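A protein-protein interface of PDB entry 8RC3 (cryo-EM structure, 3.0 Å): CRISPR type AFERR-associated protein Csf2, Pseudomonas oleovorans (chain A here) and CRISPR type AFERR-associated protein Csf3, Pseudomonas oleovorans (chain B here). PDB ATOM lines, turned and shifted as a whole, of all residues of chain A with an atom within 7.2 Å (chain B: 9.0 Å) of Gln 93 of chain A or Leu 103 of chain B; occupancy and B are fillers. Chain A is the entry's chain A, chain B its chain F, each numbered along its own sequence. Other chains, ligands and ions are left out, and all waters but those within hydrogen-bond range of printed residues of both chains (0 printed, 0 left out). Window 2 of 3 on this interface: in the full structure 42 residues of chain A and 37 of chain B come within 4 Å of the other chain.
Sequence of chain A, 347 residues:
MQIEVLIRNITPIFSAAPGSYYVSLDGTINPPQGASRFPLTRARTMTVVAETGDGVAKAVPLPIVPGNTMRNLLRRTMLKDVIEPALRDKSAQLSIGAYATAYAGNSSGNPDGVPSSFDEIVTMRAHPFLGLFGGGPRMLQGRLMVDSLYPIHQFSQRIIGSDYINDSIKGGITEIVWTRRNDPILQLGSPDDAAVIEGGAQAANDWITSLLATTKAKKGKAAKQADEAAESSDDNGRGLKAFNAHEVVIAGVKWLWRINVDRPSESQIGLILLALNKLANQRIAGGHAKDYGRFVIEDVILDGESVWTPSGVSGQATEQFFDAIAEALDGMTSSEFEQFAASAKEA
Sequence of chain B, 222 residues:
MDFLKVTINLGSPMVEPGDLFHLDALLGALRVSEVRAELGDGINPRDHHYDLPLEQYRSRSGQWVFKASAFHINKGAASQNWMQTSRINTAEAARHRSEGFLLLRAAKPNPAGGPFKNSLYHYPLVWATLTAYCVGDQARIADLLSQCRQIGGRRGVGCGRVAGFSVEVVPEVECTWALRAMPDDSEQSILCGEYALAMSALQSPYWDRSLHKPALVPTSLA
Leu 87 of chain A touches Phe 101 of chain B.
Ala 92 of chain A touches Phe 101 of chain B.
Gln 93 of chain A touches Gly 100 of chain B.
CA of Gln 93 of chain A touches O of Phe 101 of chain B, 3.5 Å away.
CD2 of Leu 103 of chain B touches OE1 of Gln 93 of chain A, at 3.2 Å.
Leu 102 of chain B touches Leu 94 of chain A (CA to O, 3.3 Å).
Ser 95 of chain A touches Leu 102 of chain B.
Ile 96 of chain A touches Leu 102 of chain B (CA to CD1, 3.7 Å).
CD1 of Leu 104 of chain B touches CG1 of Ile 96 of chain A, 3.7 Å away.
Ile 96 of chain A touches Phe 116 of chain B.
NH2 of Arg 88 of chain A lies within hydrogen-bond range of O of Glu 99 of chain B (2.7 Å).
The backbone NH of Leu 94 of chain A is in hydrogen-bond range of the backbone carbonyl oxygen of Phe 101 of chain B.
N of Leu 103 of chain B lies within hydrogen-bond range of O of Leu 94 of chain A (2.9 Å).
The backbone NH (N) of Ala 93 of chain B sits close to the side-chain hydroxyl (OH) of Tyr 99 of chain A (3.4 Å).
A ring nitrogen (ND1) of His 96 of chain B lies within hydrogen-bond range of the side-chain hydroxyl (OH) of Tyr 99 of chain A, at 2.8 Å.
Printed residues of chain B that touch a printed residue of chain A: Ala 93, His 96, Glu 99, Gly 100, Phe 101, Leu 102, Leu 103, Leu 104 and Phe 116.
Along chain B the printed residues that touch a printed residue of chain A span positions 93 to 116.
Of the 15 printed residues of chain A, 8 touch a printed residue of chain B.
Hydrophobic or aromatic side chains of chain A within 4 Å of the printed part of chain B: Leu 87, Leu 94, Ile 96 and Tyr 99.
Printed residues of chain B within 4 Å of Arg 88 of chain A: Glu 99 (2.7 Å) and Phe 101 (3.5 Å).
Of the printed residues of chain B, Gln 93 of chain A touches Gly 100 (3.1 Å), Phe 101 (3.5 Å) and Leu 103 (3.2 Å).
Of the printed residues of chain B, Ile 96 of chain A touches Leu 102, Leu 104 and Phe 116.
Ala 98 of chain A touches none of the printed residues of chain B.
Of the printed residues of chain A, His 96 of chain B touches Tyr 99.
Printed residues of chain A within 4 Å of Gly 100 of chain B: Gln 93.
Of the printed residues of chain A, Leu 102 of chain B touches Leu 94 (3.3 Å), Ser 95 (3.6 Å), Ile 96 (3.7 Å) and Tyr 99 (3.6 Å).
Leu 103 of chain B touches just these residues of chain A: Gln 93 (3.2 Å) and Leu 94 (2.9 Å).
The nearest printed residue of chain B that does not touch Ile 96 of chain A is Leu 103 of chain B (4.02 Å).
The backbone carbonyl oxygen (O) of Leu 87 of chain A is in hydrogen-bond range of the backbone NH (N) of Ala 92 of chain A, 2.8 Å away.
The side-chain hydroxyl of Ser 95 of chain A is in hydrogen-bond range of the side-chain carboxylate of Glu 338 of chain A (2.7 Å).
O of His 96 of chain B lies within hydrogen-bond range of N of Phe 101 of chain B (3.0 Å).
The backbone NH (N) of Leu 102 of chain B is in hydrogen-bond range of the backbone carbonyl oxygen (O) of His 96 of chain B.
NE of Arg 97 of chain B is in hydrogen-bond range of O of Leu 104 of chain B, at 3.2 Å.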
ATOM      1  N   LEU A  87       7.101  19.378   8.514  1.00  0.00           N
ATOM      2  CA  LEU A  87       7.296  18.534   9.685  1.00  0.00           C
ATOM      3  C   LEU A  87       6.555  19.076  10.901  1.00  0.00           C
ATOM      4  O   LEU A  87       6.070  18.294  11.724  1.00  0.00           O
ATOM      5  CB  LEU A  87       8.787  18.391   9.984  1.00  0.00           C
ATOM      6  CG  LEU A  87       9.459  17.132   9.436  1.00  0.00           C
ATOM      7  CD1 LEU A  87       9.460  17.147   7.927  1.00  0.00           C
ATOM      8  CD2 LEU A  87      10.874  17.013   9.966  1.00  0.00           C
ATOM      9  N   ARG A  88       6.464  20.402  11.037  1.00  0.00           N
ATOM     10  CA  ARG A  88       5.685  20.973  12.132  1.00  0.00           C
ATOM     11  C   ARG A  88       4.206  20.649  11.989  1.00  0.00           C
ATOM     12  O   ARG A  88       3.513  20.446  12.993  1.00  0.00           O
ATOM     13  CB  ARG A  88       5.886  22.486  12.216  1.00  0.00           C
ATOM     14  CG  ARG A  88       7.321  22.927  12.365  1.00  0.00           C
ATOM     15  CD  ARG A  88       7.937  22.337  13.613  1.00  0.00           C
ATOM     16  NE  ARG A  88       7.742  23.195  14.775  1.00  0.00           N
ATOM     17  CZ  ARG A  88       7.462  22.751  15.992  1.00  0.00           C
ATOM     18  NH1 ARG A  88       7.340  21.458  16.244  1.00  0.00           N
ATOM     19  NH2 ARG A  88       7.301  23.626  16.979  1.00  0.00           N
ATOM     20  N   LYS A  90       2.923  17.979  11.088  1.00  0.00           N
ATOM     21  CA  LYS A  90       2.755  16.661  11.685  1.00  0.00           C
ATOM     22  C   LYS A  90       3.204  16.615  13.138  1.00  0.00           C
ATOM     23  O   LYS A  90       3.170  15.540  13.745  1.00  0.00           O
ATOM     24  CB  LYS A  90       3.529  15.609  10.885  1.00  0.00           C
ATOM     25  CG  LYS A  90       3.572  15.848   9.386  1.00  0.00           C
ATOM     26  CD  LYS A  90       2.207  15.665   8.749  1.00  0.00           C
ATOM     27  CE  LYS A  90       2.277  15.840   7.242  1.00  0.00           C
ATOM     28  NZ  LYS A  90       3.243  16.901   6.844  1.00  0.00           N
ATOM     29  N   SER A  91       3.623  17.750  13.702  1.00  0.00           N
ATOM     30  CA  SER A  91       4.200  17.810  15.046  1.00  0.00           C
ATOM     31  C   SER A  91       5.417  16.897  15.164  1.00  0.00           C
ATOM     32  O   SER A  91       5.655  16.277  16.202  1.00  0.00           O
ATOM     33  CB  SER A  91       3.162  17.474  16.117  1.00  0.00           C
ATOM     34  OG  SER A  91       3.776  17.335  17.387  1.00  0.00           O
ATOM     35  N   ALA A  92       6.196  16.815  14.089  1.00  0.00           N
ATOM     36  CA  ALA A  92       7.381  15.976  14.087  1.00  0.00           C
ATOM     37  C   ALA A  92       8.469  16.578  14.965  1.00  0.00           C
ATOM     38  O   ALA A  92       8.597  17.797  15.090  1.00  0.00           O
ATOM     39  CB  ALA A  92       7.902  15.788  12.665  1.00  0.00           C
ATOM     40  N   GLN A  93       9.258  15.701  15.578  1.00  0.00           N
ATOM     41  CA  GLN A  93      10.362  16.100  16.437  1.00  0.00           C
ATOM     42  C   GLN A  93      11.629  15.436  15.929  1.00  0.00           C
ATOM     43  O   GLN A  93      11.644  14.226  15.685  1.00  0.00           O
ATOM     44  CB  GLN A  93      10.098  15.709  17.892  1.00  0.00           C
ATOM     45  CG  GLN A  93       9.211  16.688  18.630  1.00  0.00           C
ATOM     46  CD  GLN A  93       9.054  16.339  20.091  1.00  0.00           C
ATOM     47  OE1 GLN A  93       9.555  15.315  20.553  1.00  0.00           O
ATOM     48  NE2 GLN A  93       8.354  17.190  20.829  1.00  0.00           N
ATOM     49  N   LEU A  94      12.685  16.224  15.772  1.00  0.00           N
ATOM     50  CA  LEU A  94      13.943  15.748  15.221  1.00  0.00           C
ATOM     51  C   LEU A  94      14.977  15.651  16.330  1.00  0.00           C
ATOM     52  O   LEU A  94      15.145  16.590  17.112  1.00  0.00           O
ATOM     53  CB  LEU A  94      14.441  16.677  14.116  1.00  0.00           C
ATOM     54  CG  LEU A  94      13.880  16.433  12.719  1.00  0.00           C
ATOM     55  CD1 LEU A  94      14.700  17.181  11.694  1.00  0.00           C
ATOM     56  CD2 LEU A  94      13.863  14.956  12.407  1.00  0.00           C
ATOM     57  N   SER A  95      15.664  14.515  16.395  1.00  0.00           N
ATOM     58  CA  SER A  95      16.758  14.366  17.335  1.00  0.00           C
ATOM     59  C   SER A  95      17.938  15.230  16.902  1.00  0.00           C
ATOM     60  O   SER A  95      17.934  15.849  15.836  1.00  0.00           O
ATOM     61  CB  SER A  95      17.179  12.903  17.439  1.00  0.00           C
ATOM     62  OG  SER A  95      17.473  12.371  16.161  1.00  0.00           O
ATOM     63  N   ILE A  96      18.963  15.270  17.752  1.00  0.00           N
ATOM     64  CA  ILE A  96      20.130  16.090  17.446  1.00  0.00           C
ATOM     65  C   ILE A  96      20.862  15.544  16.226  1.00  0.00           C
ATOM     66  O   ILE A  96      21.334  16.309  15.377  1.00  0.00           O
ATOM     67  CB  ILE A  96      21.047  16.192  18.677  1.00  0.00           C
ATOM     68  CG1 ILE A  96      22.292  17.015  18.346  1.00  0.00           C
ATOM     69  CG2 ILE A  96      21.411  14.813  19.204  1.00  0.00           C
ATOM     70  CD1 ILE A  96      21.981  18.404  17.854  1.00  0.00           C
ATOM     71  N   GLY A  97      20.964  14.219  16.110  1.00  0.00           N
ATOM     72  CA  GLY A  97      21.621  13.640  14.949  1.00  0.00           C
ATOM     73  C   GLY A  97      20.875  13.916  13.658  1.00  0.00           C
ATOM     74  O   GLY A  97      21.476  14.304  12.652  1.00  0.00           O
ATOM     75  N   ALA A  98      19.554  13.717  13.667  1.00  0.00           N
ATOM     76  CA  ALA A  98      18.759  13.970  12.470  1.00  0.00           C
ATOM     77  C   ALA A  98      18.778  15.444  12.100  1.00  0.00           C
ATOM     78  O   ALA A  98      18.878  15.794  10.918  1.00  0.00           O
ATOM     79  CB  ALA A  98      17.325  13.488  12.680  1.00  0.00           C
ATOM     80  N   TYR A  99      18.685  16.324  13.097  1.00  0.00           N
ATOM     81  CA  TYR A  99      18.750  17.757  12.839  1.00  0.00           C
ATOM     82  C   TYR A  99      20.093  18.149  12.242  1.00  0.00           C
ATOM     83  O   TYR A  99      20.151  18.923  11.280  1.00  0.00           O
ATOM     84  CB  TYR A  99      18.493  18.520  14.137  1.00  0.00           C
ATOM     85  CG  TYR A  99      18.426  20.019  14.000  1.00  0.00           C
ATOM     86  CD1 TYR A  99      19.575  20.790  14.014  1.00  0.00           C
ATOM     87  CD2 TYR A  99      17.209  20.665  13.877  1.00  0.00           C
ATOM     88  CE1 TYR A  99      19.515  22.156  13.899  1.00  0.00           C
ATOM     89  CE2 TYR A  99      17.140  22.030  13.763  1.00  0.00           C
ATOM     90  CZ  TYR A  99      18.296  22.771  13.772  1.00  0.00           C
ATOM     91  OH  TYR A  99      18.233  24.138  13.656  1.00  0.00           O
ATOM     92  N   SER A 334       9.091  12.270  10.177  1.00  0.00           N
ATOM     93  CA  SER A 334      10.413  12.410  10.774  1.00  0.00           C
ATOM     94  C   SER A 334      11.175  11.093  10.808  1.00  0.00           C
ATOM     95  O   SER A 334      12.406  11.108  10.920  1.00  0.00           O
ATOM     96  CB  SER A 334      10.293  12.972  12.187  1.00  0.00           C
ATOM     97  OG  SER A 334       9.356  12.231  12.948  1.00  0.00           O
ATOM     98  N   SER A 335      10.474   9.961  10.715  1.00  0.00           N
ATOM     99  CA  SER A 335      11.146   8.668  10.742  1.00  0.00           C
ATOM    100  C   SER A 335      12.094   8.503   9.564  1.00  0.00           C
ATOM    101  O   SER A 335      13.133   7.849   9.694  1.00  0.00           O
ATOM    102  CB  SER A 335      10.117   7.540  10.755  1.00  0.00           C
ATOM    103  OG  SER A 335       9.334   7.584  11.934  1.00  0.00           O
ATOM    104  N   GLU A 338      15.187  10.242  10.639  1.00  0.00           N
ATOM    105  CA  GLU A 338      15.892   9.453  11.644  1.00  0.00           C
ATOM    106  C   GLU A 338      16.621   8.275  11.012  1.00  0.00           C
ATOM    107  O   GLU A 338      17.761   7.971  11.381  1.00  0.00           O
ATOM    108  CB  GLU A 338      14.916   8.964  12.712  1.00  0.00           C
ATOM    109  CG  GLU A 338      14.075  10.056  13.339  1.00  0.00           C
ATOM    110  CD  GLU A 338      14.903  11.067  14.100  1.00  0.00           C
ATOM    111  OE1 GLU A 338      15.928  10.673  14.694  1.00  0.00           O
ATOM    112  OE2 GLU A 338      14.528  12.256  14.104  1.00  0.00           O
ATOM    113  N   ALA B  93      18.843  26.960  15.531  1.00  0.00           N
ATOM    114  CA  ALA B  93      18.880  25.804  16.416  1.00  0.00           C
ATOM    115  C   ALA B  93      18.235  26.116  17.756  1.00  0.00           C
ATOM    116  O   ALA B  93      17.473  25.304  18.289  1.00  0.00           O
ATOM    117  CB  ALA B  93      20.320  25.342  16.613  1.00  0.00           C
ATOM    118  N   HIS B  96      14.438  26.309  17.263  1.00  0.00           N
ATOM    119  CA  HIS B  96      13.854  24.979  17.125  1.00  0.00           C
ATOM    120  C   HIS B  96      13.846  24.239  18.454  1.00  0.00           C
ATOM    121  O   HIS B  96      12.890  23.521  18.767  1.00  0.00           O
ATOM    122  CB  HIS B  96      14.621  24.184  16.073  1.00  0.00           C
ATOM    123  CG  HIS B  96      14.465  24.715  14.685  1.00  0.00           C
ATOM    124  ND1 HIS B  96      15.505  24.754  13.782  1.00  0.00           N
ATOM    125  CD2 HIS B  96      13.390  25.227  14.042  1.00  0.00           C
ATOM    126  CE1 HIS B  96      15.078  25.271  12.645  1.00  0.00           C
ATOM    127  NE2 HIS B  96      13.798  25.565  12.776  1.00  0.00           N
ATOM    128  N   ARG B  97      14.910  24.392  19.239  1.00  0.00           N
ATOM    129  CA  ARG B  97      14.959  23.798  20.568  1.00  0.00           C
ATOM    130  C   ARG B  97      13.856  24.355  21.454  1.00  0.00           C
ATOM    131  O   ARG B  97      13.234  23.615  22.224  1.00  0.00           O
ATOM    132  CB  ARG B  97      16.333  24.057  21.181  1.00  0.00           C
ATOM    133  CG  ARG B  97      16.645  23.287  22.436  1.00  0.00           C
ATOM    134  CD  ARG B  97      18.087  23.538  22.836  1.00  0.00           C
ATOM    135  NE  ARG B  97      18.341  23.239  24.238  1.00  0.00           N
ATOM    136  CZ  ARG B  97      18.006  24.034  25.243  1.00  0.00           C
ATOM    137  NH1 ARG B  97      17.372  25.176  25.038  1.00  0.00           N
ATOM    138  NH2 ARG B  97      18.316  23.676  26.485  1.00  0.00           N
ATOM    139  N   SER B  98      13.606  25.662  21.362  1.00  0.00           N
ATOM    140  CA  SER B  98      12.532  26.274  22.137  1.00  0.00           C
ATOM    141  C   SER B  98      11.167  25.753  21.708  1.00  0.00           C
ATOM    142  O   SER B  98      10.313  25.462  22.553  1.00  0.00           O
ATOM    143  CB  SER B  98      12.589  27.793  21.994  1.00  0.00           C
ATOM    144  OG  SER B  98      11.339  28.380  22.307  1.00  0.00           O
ATOM    145  N   GLU B  99      10.941  25.628  20.404  1.00  0.00           N
ATOM    146  CA  GLU B  99       9.637  25.254  19.873  1.00  0.00           C
ATOM    147  C   GLU B  99       9.410  23.751  19.843  1.00  0.00           C
ATOM    148  O   GLU B  99       8.319  23.314  19.467  1.00  0.00           O
ATOM    149  CB  GLU B  99       9.457  25.826  18.466  1.00  0.00           C
ATOM    150  CG  GLU B  99       8.869  27.222  18.443  1.00  0.00           C
ATOM    151  CD  GLU B  99       9.516  28.102  17.400  1.00  0.00           C
ATOM    152  OE1 GLU B  99      10.156  27.555  16.479  1.00  0.00           O
ATOM    153  OE2 GLU B  99       9.382  29.340  17.498  1.00  0.00           O
ATOM    154  N   GLY B 100      10.403  22.954  20.225  1.00  0.00           N
ATOM    155  CA  GLY B 100      10.244  21.519  20.294  1.00  0.00           C
ATOM    156  C   GLY B 100      10.546  20.764  19.021  1.00  0.00           C
ATOM    157  O   GLY B 100      10.447  19.532  19.019  1.00  0.00           O
ATOM    158  N   PHE B 101      10.903  21.453  17.937  1.00  0.00           N
ATOM    159  CA  PHE B 101      11.281  20.756  16.713  1.00  0.00           C
ATOM    160  C   PHE B 101      12.525  19.906  16.927  1.00  0.00           C
ATOM    161  O   PHE B 101      12.606  18.772  16.442  1.00  0.00           O
ATOM    162  CB  PHE B 101      11.510  21.762  15.588  1.00  0.00           C
ATOM    163  CG  PHE B 101      11.752  21.132  14.249  1.00  0.00           C
ATOM    164  CD1 PHE B 101      10.797  20.331  13.660  1.00  0.00           C
ATOM    165  CD2 PHE B 101      12.939  21.348  13.578  1.00  0.00           C
ATOM    166  CE1 PHE B 101      11.023  19.760  12.430  1.00  0.00           C
ATOM    167  CE2 PHE B 101      13.168  20.778  12.350  1.00  0.00           C
ATOM    168  CZ  PHE B 101      12.208  19.985  11.775  1.00  0.00           C
ATOM    169  N   LEU B 102      13.501  20.435  17.653  1.00  0.00           N
ATOM    170  CA  LEU B 102      14.745  19.738  17.940  1.00  0.00           C
ATOM    171  C   LEU B 102      14.737  19.288  19.393  1.00  0.00           C
ATOM    172  O   LEU B 102      14.397  20.069  20.286  1.00  0.00           O
ATOM    173  CB  LEU B 102      15.948  20.641  17.664  1.00  0.00           C
ATOM    174  CG  LEU B 102      17.272  20.231  18.300  1.00  0.00           C
ATOM    175  CD1 LEU B 102      17.803  18.967  17.659  1.00  0.00           C
ATOM    176  CD2 LEU B 102      18.283  21.352  18.194  1.00  0.00           C
ATOM    177  N   LEU B 103      15.099  18.030  19.623  1.00  0.00           N
ATOM    178  CA  LEU B 103      15.164  17.463  20.968  1.00  0.00           C
ATOM    179  C   LEU B 103      16.618  17.502  21.422  1.00  0.00           C
ATOM    180  O   LEU B 103      17.380  16.558  21.216  1.00  0.00           O
ATOM    181  CB  LEU B 103      14.606  16.047  20.991  1.00  0.00           C
ATOM    182  CG  LEU B 103      13.173  15.908  20.480  1.00  0.00           C
ATOM    183  CD1 LEU B 103      12.710  14.467  20.564  1.00  0.00           C
ATOM    184  CD2 LEU B 103      12.258  16.817  21.276  1.00  0.00           C
ATOM    185  N   LEU B 104      17.003  18.611  22.045  1.00  0.00           N
ATOM    186  CA  LEU B 104      18.340  18.771  22.595  1.00  0.00           C
ATOM    187  C   LEU B 104      18.225  19.270  24.025  1.00  0.00           C
ATOM    188  O   LEU B 104      17.439  20.178  24.308  1.00  0.00           O
ATOM    189  CB  LEU B 104      19.176  19.742  21.758  1.00  0.00           C
ATOM    190  CG  LEU B 104      20.664  19.775  22.101  1.00  0.00           C
ATOM    191  CD1 LEU B 104      21.348  18.503  21.639  1.00  0.00           C
ATOM    192  CD2 LEU B 104      21.325  20.989  21.490  1.00  0.00           C
ATOM    193  N   ARG B 105      19.005  18.672  24.925  1.00  0.00           N
ATOM    194  CA  ARG B 105      19.021  19.088  26.318  1.00  0.00           C
ATOM    195  C   ARG B 105      20.227  19.949  26.664  1.00  0.00           C
ATOM    196  O   ARG B 105      20.183  20.680  27.659  1.00  0.00           O
ATOM    197  CB  ARG B 105      18.983  17.856  27.234  1.00  0.00           C
ATOM    198  CG  ARG B 105      18.879  18.169  28.720  1.00  0.00           C
ATOM    199  CD  ARG B 105      18.205  17.052  29.493  1.00  0.00           C
ATOM    200  NE  ARG B 105      18.486  15.737  28.931  1.00  0.00           N
ATOM    201  CZ  ARG B 105      19.353  14.876  29.444  1.00  0.00           C
ATOM    202  NH1 ARG B 105      20.061  15.167  30.522  1.00  0.00           N
ATOM    203  NH2 ARG B 105      19.515  13.693  28.859  1.00  0.00           N
ATOM    204  N   ALA B 106      21.285  19.899  25.858  1.00  0.00           N
ATOM    205  CA  ALA B 106      22.477  20.688  26.130  1.00  0.00           C
ATOM    206  C   ALA B 106      22.147  22.174  26.147  1.00  0.00           C
ATOM    207  O   ALA B 106      21.372  22.667  25.324  1.00  0.00           O
ATOM    208  CB  ALA B 106      23.552  20.400  25.085  1.00  0.00           C
ATOM    209  N   PHE B 116      27.301  21.072  16.863  1.00  0.00           N
ATOM    210  CA  PHE B 116      27.332  22.476  16.461  1.00  0.00           C
ATOM    211  C   PHE B 116      28.753  22.986  16.292  1.00  0.00           C
ATOM    212  O   PHE B 116      29.050  24.139  16.609  1.00  0.00           O
ATOM    213  CB  PHE B 116      26.573  23.329  17.470  1.00  0.00           C
ATOM    214  CG  PHE B 116      25.113  23.022  17.533  1.00  0.00           C
ATOM    215  CD1 PHE B 116      24.273  23.405  16.511  1.00  0.00           C
ATOM    216  CD2 PHE B 116      24.582  22.337  18.606  1.00  0.00           C
ATOM    217  CE1 PHE B 116      22.933  23.118  16.559  1.00  0.00           C
ATOM    218  CE2 PHE B 116      23.239  22.052  18.658  1.00  0.00           C
ATOM    219  CZ  PHE B 116      22.415  22.442  17.634  1.00  0.00           C
